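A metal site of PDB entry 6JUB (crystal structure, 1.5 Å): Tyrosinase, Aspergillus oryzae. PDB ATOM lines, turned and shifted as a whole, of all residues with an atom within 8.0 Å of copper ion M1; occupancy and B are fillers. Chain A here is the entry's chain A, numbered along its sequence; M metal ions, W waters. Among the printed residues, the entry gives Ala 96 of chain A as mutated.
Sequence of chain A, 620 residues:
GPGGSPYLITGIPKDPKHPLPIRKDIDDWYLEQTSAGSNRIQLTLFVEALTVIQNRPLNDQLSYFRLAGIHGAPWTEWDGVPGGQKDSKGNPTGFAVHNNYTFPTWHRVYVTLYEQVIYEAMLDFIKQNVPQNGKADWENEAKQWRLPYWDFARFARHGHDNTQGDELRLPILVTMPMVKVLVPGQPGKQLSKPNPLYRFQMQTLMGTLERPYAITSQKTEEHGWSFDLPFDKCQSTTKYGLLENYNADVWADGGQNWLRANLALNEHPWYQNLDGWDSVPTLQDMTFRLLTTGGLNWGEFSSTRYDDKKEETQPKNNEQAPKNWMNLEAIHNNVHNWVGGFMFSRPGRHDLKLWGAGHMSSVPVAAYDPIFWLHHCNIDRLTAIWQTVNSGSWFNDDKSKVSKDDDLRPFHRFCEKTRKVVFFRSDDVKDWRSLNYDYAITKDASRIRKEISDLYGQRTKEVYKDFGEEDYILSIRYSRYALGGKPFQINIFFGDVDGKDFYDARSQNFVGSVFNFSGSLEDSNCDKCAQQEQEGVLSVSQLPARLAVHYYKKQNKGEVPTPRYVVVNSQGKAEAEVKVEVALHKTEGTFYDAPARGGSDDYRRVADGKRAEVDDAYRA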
ATOM      1  N   HIS A  71       0.978 -29.475 -26.287  1.00  0.00           N
ATOM      2  CA  HIS A  71       0.634 -28.492 -27.287  1.00  0.00           C
ATOM      3  C   HIS A  71       0.436 -29.117 -28.657  1.00  0.00           C
ATOM      4  O   HIS A  71      -0.482 -28.718 -29.377  1.00  0.00           O
ATOM      5  CB  HIS A  71       1.705 -27.397 -27.329  1.00  0.00           C
ATOM      6  CG  HIS A  71       1.371 -26.200 -28.169  1.00  0.00           C
ATOM      7  ND1 HIS A  71       1.934 -25.965 -29.405  1.00  0.00           N
ATOM      8  CD2 HIS A  71       0.523 -25.155 -27.953  1.00  0.00           C
ATOM      9  CE1 HIS A  71       1.454 -24.838 -29.908  1.00  0.00           C
ATOM     10  NE2 HIS A  71       0.588 -24.324 -29.043  1.00  0.00           N
ATOM     11  N   GLY A  72       1.303 -30.064 -29.036  1.00  0.00           N
ATOM     12  CA  GLY A  72       1.306 -30.601 -30.391  1.00  0.00           C
ATOM     13  C   GLY A  72       1.929 -31.980 -30.469  1.00  0.00           C
ATOM     14  O   GLY A  72       1.475 -32.898 -29.771  1.00  0.00           O
ATOM     15  N   PHE A  95      -3.758 -30.822 -28.364  1.00  0.00           N
ATOM     16  CA  PHE A  95      -4.769 -30.267 -27.474  1.00  0.00           C
ATOM     17  C   PHE A  95      -4.915 -28.757 -27.689  1.00  0.00           C
ATOM     18  O   PHE A  95      -5.962 -28.209 -27.361  1.00  0.00           O
ATOM     19  CB  PHE A  95      -4.417 -30.566 -26.020  1.00  0.00           C
ATOM     20  CG  PHE A  95      -4.576 -31.999 -25.580  1.00  0.00           C
ATOM     21  CD1 PHE A  95      -5.825 -32.601 -25.483  1.00  0.00           C
ATOM     22  CD2 PHE A  95      -3.465 -32.767 -25.237  1.00  0.00           C
ATOM     23  CE1 PHE A  95      -5.967 -33.914 -25.060  1.00  0.00           C
ATOM     24  CE2 PHE A  95      -3.598 -34.079 -24.810  1.00  0.00           C
ATOM     25  CZ  PHE A  95      -4.856 -34.653 -24.717  1.00  0.00           C
ATOM     26  N   ALA A  96      -3.851 -28.127 -28.193  1.00  0.00           N
ATOM     27  CA  ALA A  96      -3.807 -26.677 -28.295  1.00  0.00           C
ATOM     28  C   ALA A  96      -4.941 -26.127 -29.148  1.00  0.00           C
ATOM     29  O   ALA A  96      -5.302 -26.687 -30.197  1.00  0.00           O
ATOM     30  CB  ALA A  96      -2.460 -26.235 -28.877  1.00  0.00           C
ATOM     31  N   VAL A  97      -5.511 -25.013 -28.701  1.00  0.00           N
ATOM     32  CA  VAL A  97      -6.532 -24.341 -29.494  1.00  0.00           C
ATOM     33  C   VAL A  97      -5.910 -23.195 -30.301  1.00  0.00           C
ATOM     34  O   VAL A  97      -5.332 -22.270 -29.729  1.00  0.00           O
ATOM     35  CB  VAL A  97      -7.668 -23.745 -28.646  1.00  0.00           C
ATOM     36  CG1 VAL A  97      -8.609 -22.960 -29.543  1.00  0.00           C
ATOM     37  CG2 VAL A  97      -8.415 -24.843 -27.906  1.00  0.00           C
ATOM     38  N   HIS A  98      -6.078 -23.281 -31.613  1.00  0.00           N
ATOM     39  CA  HIS A  98      -5.654 -22.210 -32.512  1.00  0.00           C
ATOM     40  C   HIS A  98      -6.795 -21.873 -33.461  1.00  0.00           C
ATOM     41  O   HIS A  98      -7.611 -22.749 -33.761  1.00  0.00           O
ATOM     42  CB  HIS A  98      -4.388 -22.598 -33.292  1.00  0.00           C
ATOM     43  CG  HIS A  98      -3.238 -22.949 -32.385  1.00  0.00           C
ATOM     44  ND1 HIS A  98      -2.680 -24.207 -32.329  1.00  0.00           N
ATOM     45  CD2 HIS A  98      -2.558 -22.203 -31.484  1.00  0.00           C
ATOM     46  CE1 HIS A  98      -1.706 -24.214 -31.436  1.00  0.00           C
ATOM     47  NE2 HIS A  98      -1.602 -23.012 -30.901  1.00  0.00           N
ATOM     48  N   PHE A 103      -8.625 -19.437 -27.988  1.00  0.00           N
ATOM     49  CA  PHE A 103      -7.161 -19.377 -28.052  1.00  0.00           C
ATOM     50  C   PHE A 103      -6.556 -18.720 -26.819  1.00  0.00           C
ATOM     51  O   PHE A 103      -5.613 -19.303 -26.243  1.00  0.00           O
ATOM     52  CB  PHE A 103      -6.721 -18.677 -29.348  1.00  0.00           C
ATOM     53  CG  PHE A 103      -5.304 -18.156 -29.304  1.00  0.00           C
ATOM     54  CD1 PHE A 103      -4.206 -18.979 -29.521  1.00  0.00           C
ATOM     55  CD2 PHE A 103      -5.049 -16.821 -29.050  1.00  0.00           C
ATOM     56  CE1 PHE A 103      -2.918 -18.488 -29.459  1.00  0.00           C
ATOM     57  CE2 PHE A 103      -3.759 -16.309 -28.994  1.00  0.00           C
ATOM     58  CZ  PHE A 103      -2.678 -17.146 -29.219  1.00  0.00           C
ATOM     59  N   TRP A 106      -7.403 -21.130 -23.458  1.00  0.00           N
ATOM     60  CA  TRP A 106      -6.669 -22.393 -23.422  1.00  0.00           C
ATOM     61  C   TRP A 106      -5.224 -22.095 -23.052  1.00  0.00           C
ATOM     62  O   TRP A 106      -4.637 -22.758 -22.181  1.00  0.00           O
ATOM     63  CB  TRP A 106      -6.772 -23.150 -24.755  1.00  0.00           C
ATOM     64  CG  TRP A 106      -6.187 -24.528 -24.632  1.00  0.00           C
ATOM     65  CD1 TRP A 106      -6.859 -25.686 -24.309  1.00  0.00           C
ATOM     66  CD2 TRP A 106      -4.814 -24.894 -24.816  1.00  0.00           C
ATOM     67  NE1 TRP A 106      -5.983 -26.750 -24.301  1.00  0.00           N
ATOM     68  CE2 TRP A 106      -4.714 -26.284 -24.599  1.00  0.00           C
ATOM     69  CE3 TRP A 106      -3.654 -24.190 -25.150  1.00  0.00           C
ATOM     70  CZ2 TRP A 106      -3.512 -26.977 -24.689  1.00  0.00           C
ATOM     71  CZ3 TRP A 106      -2.451 -24.883 -25.240  1.00  0.00           C
ATOM     72  CH2 TRP A 106      -2.388 -26.266 -25.017  1.00  0.00           C
ATOM     73  N   HIS A 107      -4.612 -21.090 -23.690  1.00  0.00           N
ATOM     74  CA  HIS A 107      -3.190 -20.857 -23.385  1.00  0.00           C
ATOM     75  C   HIS A 107      -3.007 -20.232 -22.006  1.00  0.00           C
ATOM     76  O   HIS A 107      -1.954 -20.418 -21.395  1.00  0.00           O
ATOM     77  CB  HIS A 107      -2.523 -19.996 -24.466  1.00  0.00           C
ATOM     78  CG  HIS A 107      -2.366 -20.743 -25.764  1.00  0.00           C
ATOM     79  ND1 HIS A 107      -3.369 -20.850 -26.685  1.00  0.00           N
ATOM     80  CD2 HIS A 107      -1.307 -21.399 -26.280  1.00  0.00           C
ATOM     81  CE1 HIS A 107      -2.950 -21.562 -27.720  1.00  0.00           C
ATOM     82  NE2 HIS A 107      -1.693 -21.911 -27.490  1.00  0.00           N
ATOM     83  N   TYR A 110      -2.662 -23.226 -19.873  1.00  0.00           N
ATOM     84  CA  TYR A 110      -1.400 -23.906 -20.185  1.00  0.00           C
ATOM     85  C   TYR A 110      -0.194 -23.234 -19.530  1.00  0.00           C
ATOM     86  O   TYR A 110       0.702 -23.910 -19.014  1.00  0.00           O
ATOM     87  CB  TYR A 110      -1.139 -23.876 -21.687  1.00  0.00           C
ATOM     88  CG  TYR A 110      -0.146 -24.838 -22.288  1.00  0.00           C
ATOM     89  CD1 TYR A 110       0.206 -26.051 -21.720  1.00  0.00           C
ATOM     90  CD2 TYR A 110       0.435 -24.504 -23.516  1.00  0.00           C
ATOM     91  CE1 TYR A 110       1.138 -26.908 -22.311  1.00  0.00           C
ATOM     92  CE2 TYR A 110       1.330 -25.347 -24.124  1.00  0.00           C
ATOM     93  CZ  TYR A 110       1.688 -26.546 -23.523  1.00  0.00           C
ATOM     94  OH  TYR A 110       2.576 -27.354 -24.189  1.00  0.00           O
ATOM     95  N   GLU A 329      -4.196 -13.132 -31.741  1.00  0.00           N
ATOM     96  CA  GLU A 329      -3.597 -14.346 -32.268  1.00  0.00           C
ATOM     97  C   GLU A 329      -2.697 -14.042 -33.449  1.00  0.00           C
ATOM     98  O   GLU A 329      -1.628 -14.652 -33.586  1.00  0.00           O
ATOM     99  CB  GLU A 329      -4.695 -15.353 -32.622  1.00  0.00           C
ATOM    100  CG  GLU A 329      -4.126 -16.756 -32.888  1.00  0.00           C
ATOM    101  CD  GLU A 329      -5.209 -17.783 -33.133  1.00  0.00           C
ATOM    102  OE1 GLU A 329      -6.398 -17.438 -33.199  1.00  0.00           O
ATOM    103  OE2 GLU A 329      -4.850 -18.975 -33.265  1.00  0.00           O
ATOM    104  N   HIS A 332       0.610 -12.736 -32.258  1.00  0.00           N
ATOM    105  CA  HIS A 332       1.296 -13.889 -31.674  1.00  0.00           C
ATOM    106  C   HIS A 332       1.889 -14.790 -32.744  1.00  0.00           C
ATOM    107  O   HIS A 332       2.976 -15.362 -32.568  1.00  0.00           O
ATOM    108  CB  HIS A 332       0.337 -14.648 -30.754  1.00  0.00           C
ATOM    109  CG  HIS A 332       0.389 -16.133 -30.786  1.00  0.00           C
ATOM    110  ND1 HIS A 332      -0.150 -16.900 -31.800  1.00  0.00           N
ATOM    111  CD2 HIS A 332       0.882 -17.023 -29.896  1.00  0.00           C
ATOM    112  CE1 HIS A 332       0.033 -18.189 -31.530  1.00  0.00           C
ATOM    113  NE2 HIS A 332       0.665 -18.297 -30.375  1.00  0.00           N
ATOM    114  N   ASN A 333       1.203 -14.902 -33.869  1.00  0.00           N
ATOM    115  CA  ASN A 333       1.672 -15.770 -34.957  1.00  0.00           C
ATOM    116  C   ASN A 333       2.932 -15.180 -35.572  1.00  0.00           C
ATOM    117  O   ASN A 333       3.887 -15.885 -35.864  1.00  0.00           O
ATOM    118  CB  ASN A 333       0.606 -15.907 -36.049  1.00  0.00           C
ATOM    119  CG  ASN A 333      -0.573 -16.767 -35.691  1.00  0.00           C
ATOM    120  OD1 ASN A 333      -0.585 -17.472 -34.671  1.00  0.00           O
ATOM    121  ND2 ASN A 333      -1.617 -16.711 -36.531  1.00  0.00           N
ATOM    122  N   HIS A 336       5.935 -15.834 -33.329  1.00  0.00           N
ATOM    123  CA  HIS A 336       6.422 -17.202 -33.517  1.00  0.00           C
ATOM    124  C   HIS A 336       7.403 -17.321 -34.689  1.00  0.00           C
ATOM    125  O   HIS A 336       8.481 -17.893 -34.565  1.00  0.00           O
ATOM    126  CB  HIS A 336       5.224 -18.138 -33.730  1.00  0.00           C
ATOM    127  CG  HIS A 336       4.666 -18.791 -32.513  1.00  0.00           C
ATOM    128  ND1 HIS A 336       5.290 -19.830 -31.850  1.00  0.00           N
ATOM    129  CD2 HIS A 336       3.523 -18.579 -31.823  1.00  0.00           C
ATOM    130  CE1 HIS A 336       4.559 -20.211 -30.816  1.00  0.00           C
ATOM    131  NE2 HIS A 336       3.480 -19.474 -30.778  1.00  0.00           N
ATOM    132  N   VAL A 363       3.865 -24.996 -35.361  1.00  0.00           N
ATOM    133  CA  VAL A 363       2.881 -25.395 -34.352  1.00  0.00           C
ATOM    134  C   VAL A 363       3.183 -26.706 -33.651  1.00  0.00           C
ATOM    135  O   VAL A 363       3.103 -26.773 -32.415  1.00  0.00           O
ATOM    136  CB  VAL A 363       1.475 -25.461 -34.978  1.00  0.00           C
ATOM    137  CG1 VAL A 363       0.502 -26.008 -33.940  1.00  0.00           C
ATOM    138  CG2 VAL A 363       1.043 -24.093 -35.475  1.00  0.00           C
ATOM    139  N   ALA A 366       6.663 -25.997 -31.486  1.00  0.00           N
ATOM    140  CA  ALA A 366       7.037 -24.707 -30.918  1.00  0.00           C
ATOM    141  C   ALA A 366       7.154 -24.760 -29.396  1.00  0.00           C
ATOM    142  O   ALA A 366       8.018 -24.065 -28.838  1.00  0.00           O
ATOM    143  CB  ALA A 366       6.063 -23.606 -31.332  1.00  0.00           C
ATOM    144  N   ALA A 367       6.321 -25.542 -28.720  1.00  0.00           N
ATOM    145  CA  ALA A 367       6.329 -25.527 -27.249  1.00  0.00           C
ATOM    146  C   ALA A 367       7.610 -26.085 -26.663  1.00  0.00           C
ATOM    147  O   ALA A 367       7.906 -25.850 -25.487  1.00  0.00           O
ATOM    148  CB  ALA A 367       5.116 -26.294 -26.729  1.00  0.00           C
ATOM    149  N   PHE A 372       8.920 -20.232 -25.762  1.00  0.00           N
ATOM    150  CA  PHE A 372       7.491 -20.373 -26.032  1.00  0.00           C
ATOM    151  C   PHE A 372       6.645 -19.905 -24.853  1.00  0.00           C
ATOM    152  O   PHE A 372       5.652 -19.191 -25.000  1.00  0.00           O
ATOM    153  CB  PHE A 372       7.199 -21.851 -26.319  1.00  0.00           C
ATOM    154  CG  PHE A 372       5.737 -22.160 -26.416  1.00  0.00           C
ATOM    155  CD1 PHE A 372       5.005 -22.498 -25.289  1.00  0.00           C
ATOM    156  CD2 PHE A 372       5.084 -22.124 -27.643  1.00  0.00           C
ATOM    157  CE1 PHE A 372       3.643 -22.792 -25.387  1.00  0.00           C
ATOM    158  CE2 PHE A 372       3.734 -22.411 -27.743  1.00  0.00           C
ATOM    159  CZ  PHE A 372       3.006 -22.755 -26.622  1.00  0.00           C
ATOM    160  N   HIS A 376       4.068 -16.830 -24.533  1.00  0.00           N
ATOM    161  CA  HIS A 376       2.672 -17.028 -24.139  1.00  0.00           C
ATOM    162  C   HIS A 376       2.363 -16.339 -22.819  1.00  0.00           C
ATOM    163  O   HIS A 376       1.201 -15.977 -22.592  1.00  0.00           O
ATOM    164  CB  HIS A 376       2.284 -18.518 -24.128  1.00  0.00           C
ATOM    165  CG  HIS A 376       1.780 -18.835 -25.517  1.00  0.00           C
ATOM    166  ND1 HIS A 376       0.526 -18.473 -25.965  1.00  0.00           N
ATOM    167  CD2 HIS A 376       2.418 -19.410 -26.552  1.00  0.00           C
ATOM    168  CE1 HIS A 376       0.392 -18.863 -27.221  1.00  0.00           C
ATOM    169  NE2 HIS A 376       1.526 -19.432 -27.594  1.00  0.00           N
ATOM    170  N   PHE A 517       0.666 -19.415 -38.973  1.00  0.00           N
ATOM    171  CA  PHE A 517       1.139 -20.361 -37.967  1.00  0.00           C
ATOM    172  C   PHE A 517       0.229 -21.589 -37.982  1.00  0.00           C
ATOM    173  O   PHE A 517      -0.806 -21.631 -37.303  1.00  0.00           O
ATOM    174  CB  PHE A 517       1.129 -19.697 -36.600  1.00  0.00           C
ATOM    175  CG  PHE A 517       1.769 -20.448 -35.462  1.00  0.00           C
ATOM    176  CD1 PHE A 517       3.071 -20.892 -35.515  1.00  0.00           C
ATOM    177  CD2 PHE A 517       1.027 -20.680 -34.317  1.00  0.00           C
ATOM    178  CE1 PHE A 517       3.628 -21.553 -34.440  1.00  0.00           C
ATOM    179  CE2 PHE A 517       1.584 -21.341 -33.242  1.00  0.00           C
ATOM    180  CZ  PHE A 517       2.895 -21.770 -33.290  1.00  0.00           C
HETATM  181 CU    CU M   1      -0.482 -22.669 -29.129  1.00  0.00          CU
HETATM  182 CU    CU M   2       1.786 -19.725 -29.649  1.00  0.00          CU
HETATM  183  O   HOH W   1       1.295 -21.464 -29.692  1.00  0.00           O
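ND1 of His 107 is in hydrogen-bond range of O of Phe 103 (2.8 Å).
The backbone NH (N) of His 71 sits close to the side-chain hydroxyl (OH) of Tyr 110 (3.4 Å).
The backbone carbonyl oxygen (O) of Val 363 is in hydrogen-bond range of a ring nitrogen (ND1) of His 71, at 3.3 Å.
Copper ion M1 is bound by NE2 of His 71 (2.0 Å), NE2 of His 98 (2.1 Å), NE2 of His 107 (2.2 Å) and water W1 (2.2 Å).
Within 4 Å of copper ion M1: His 71, His 98 and His 107.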
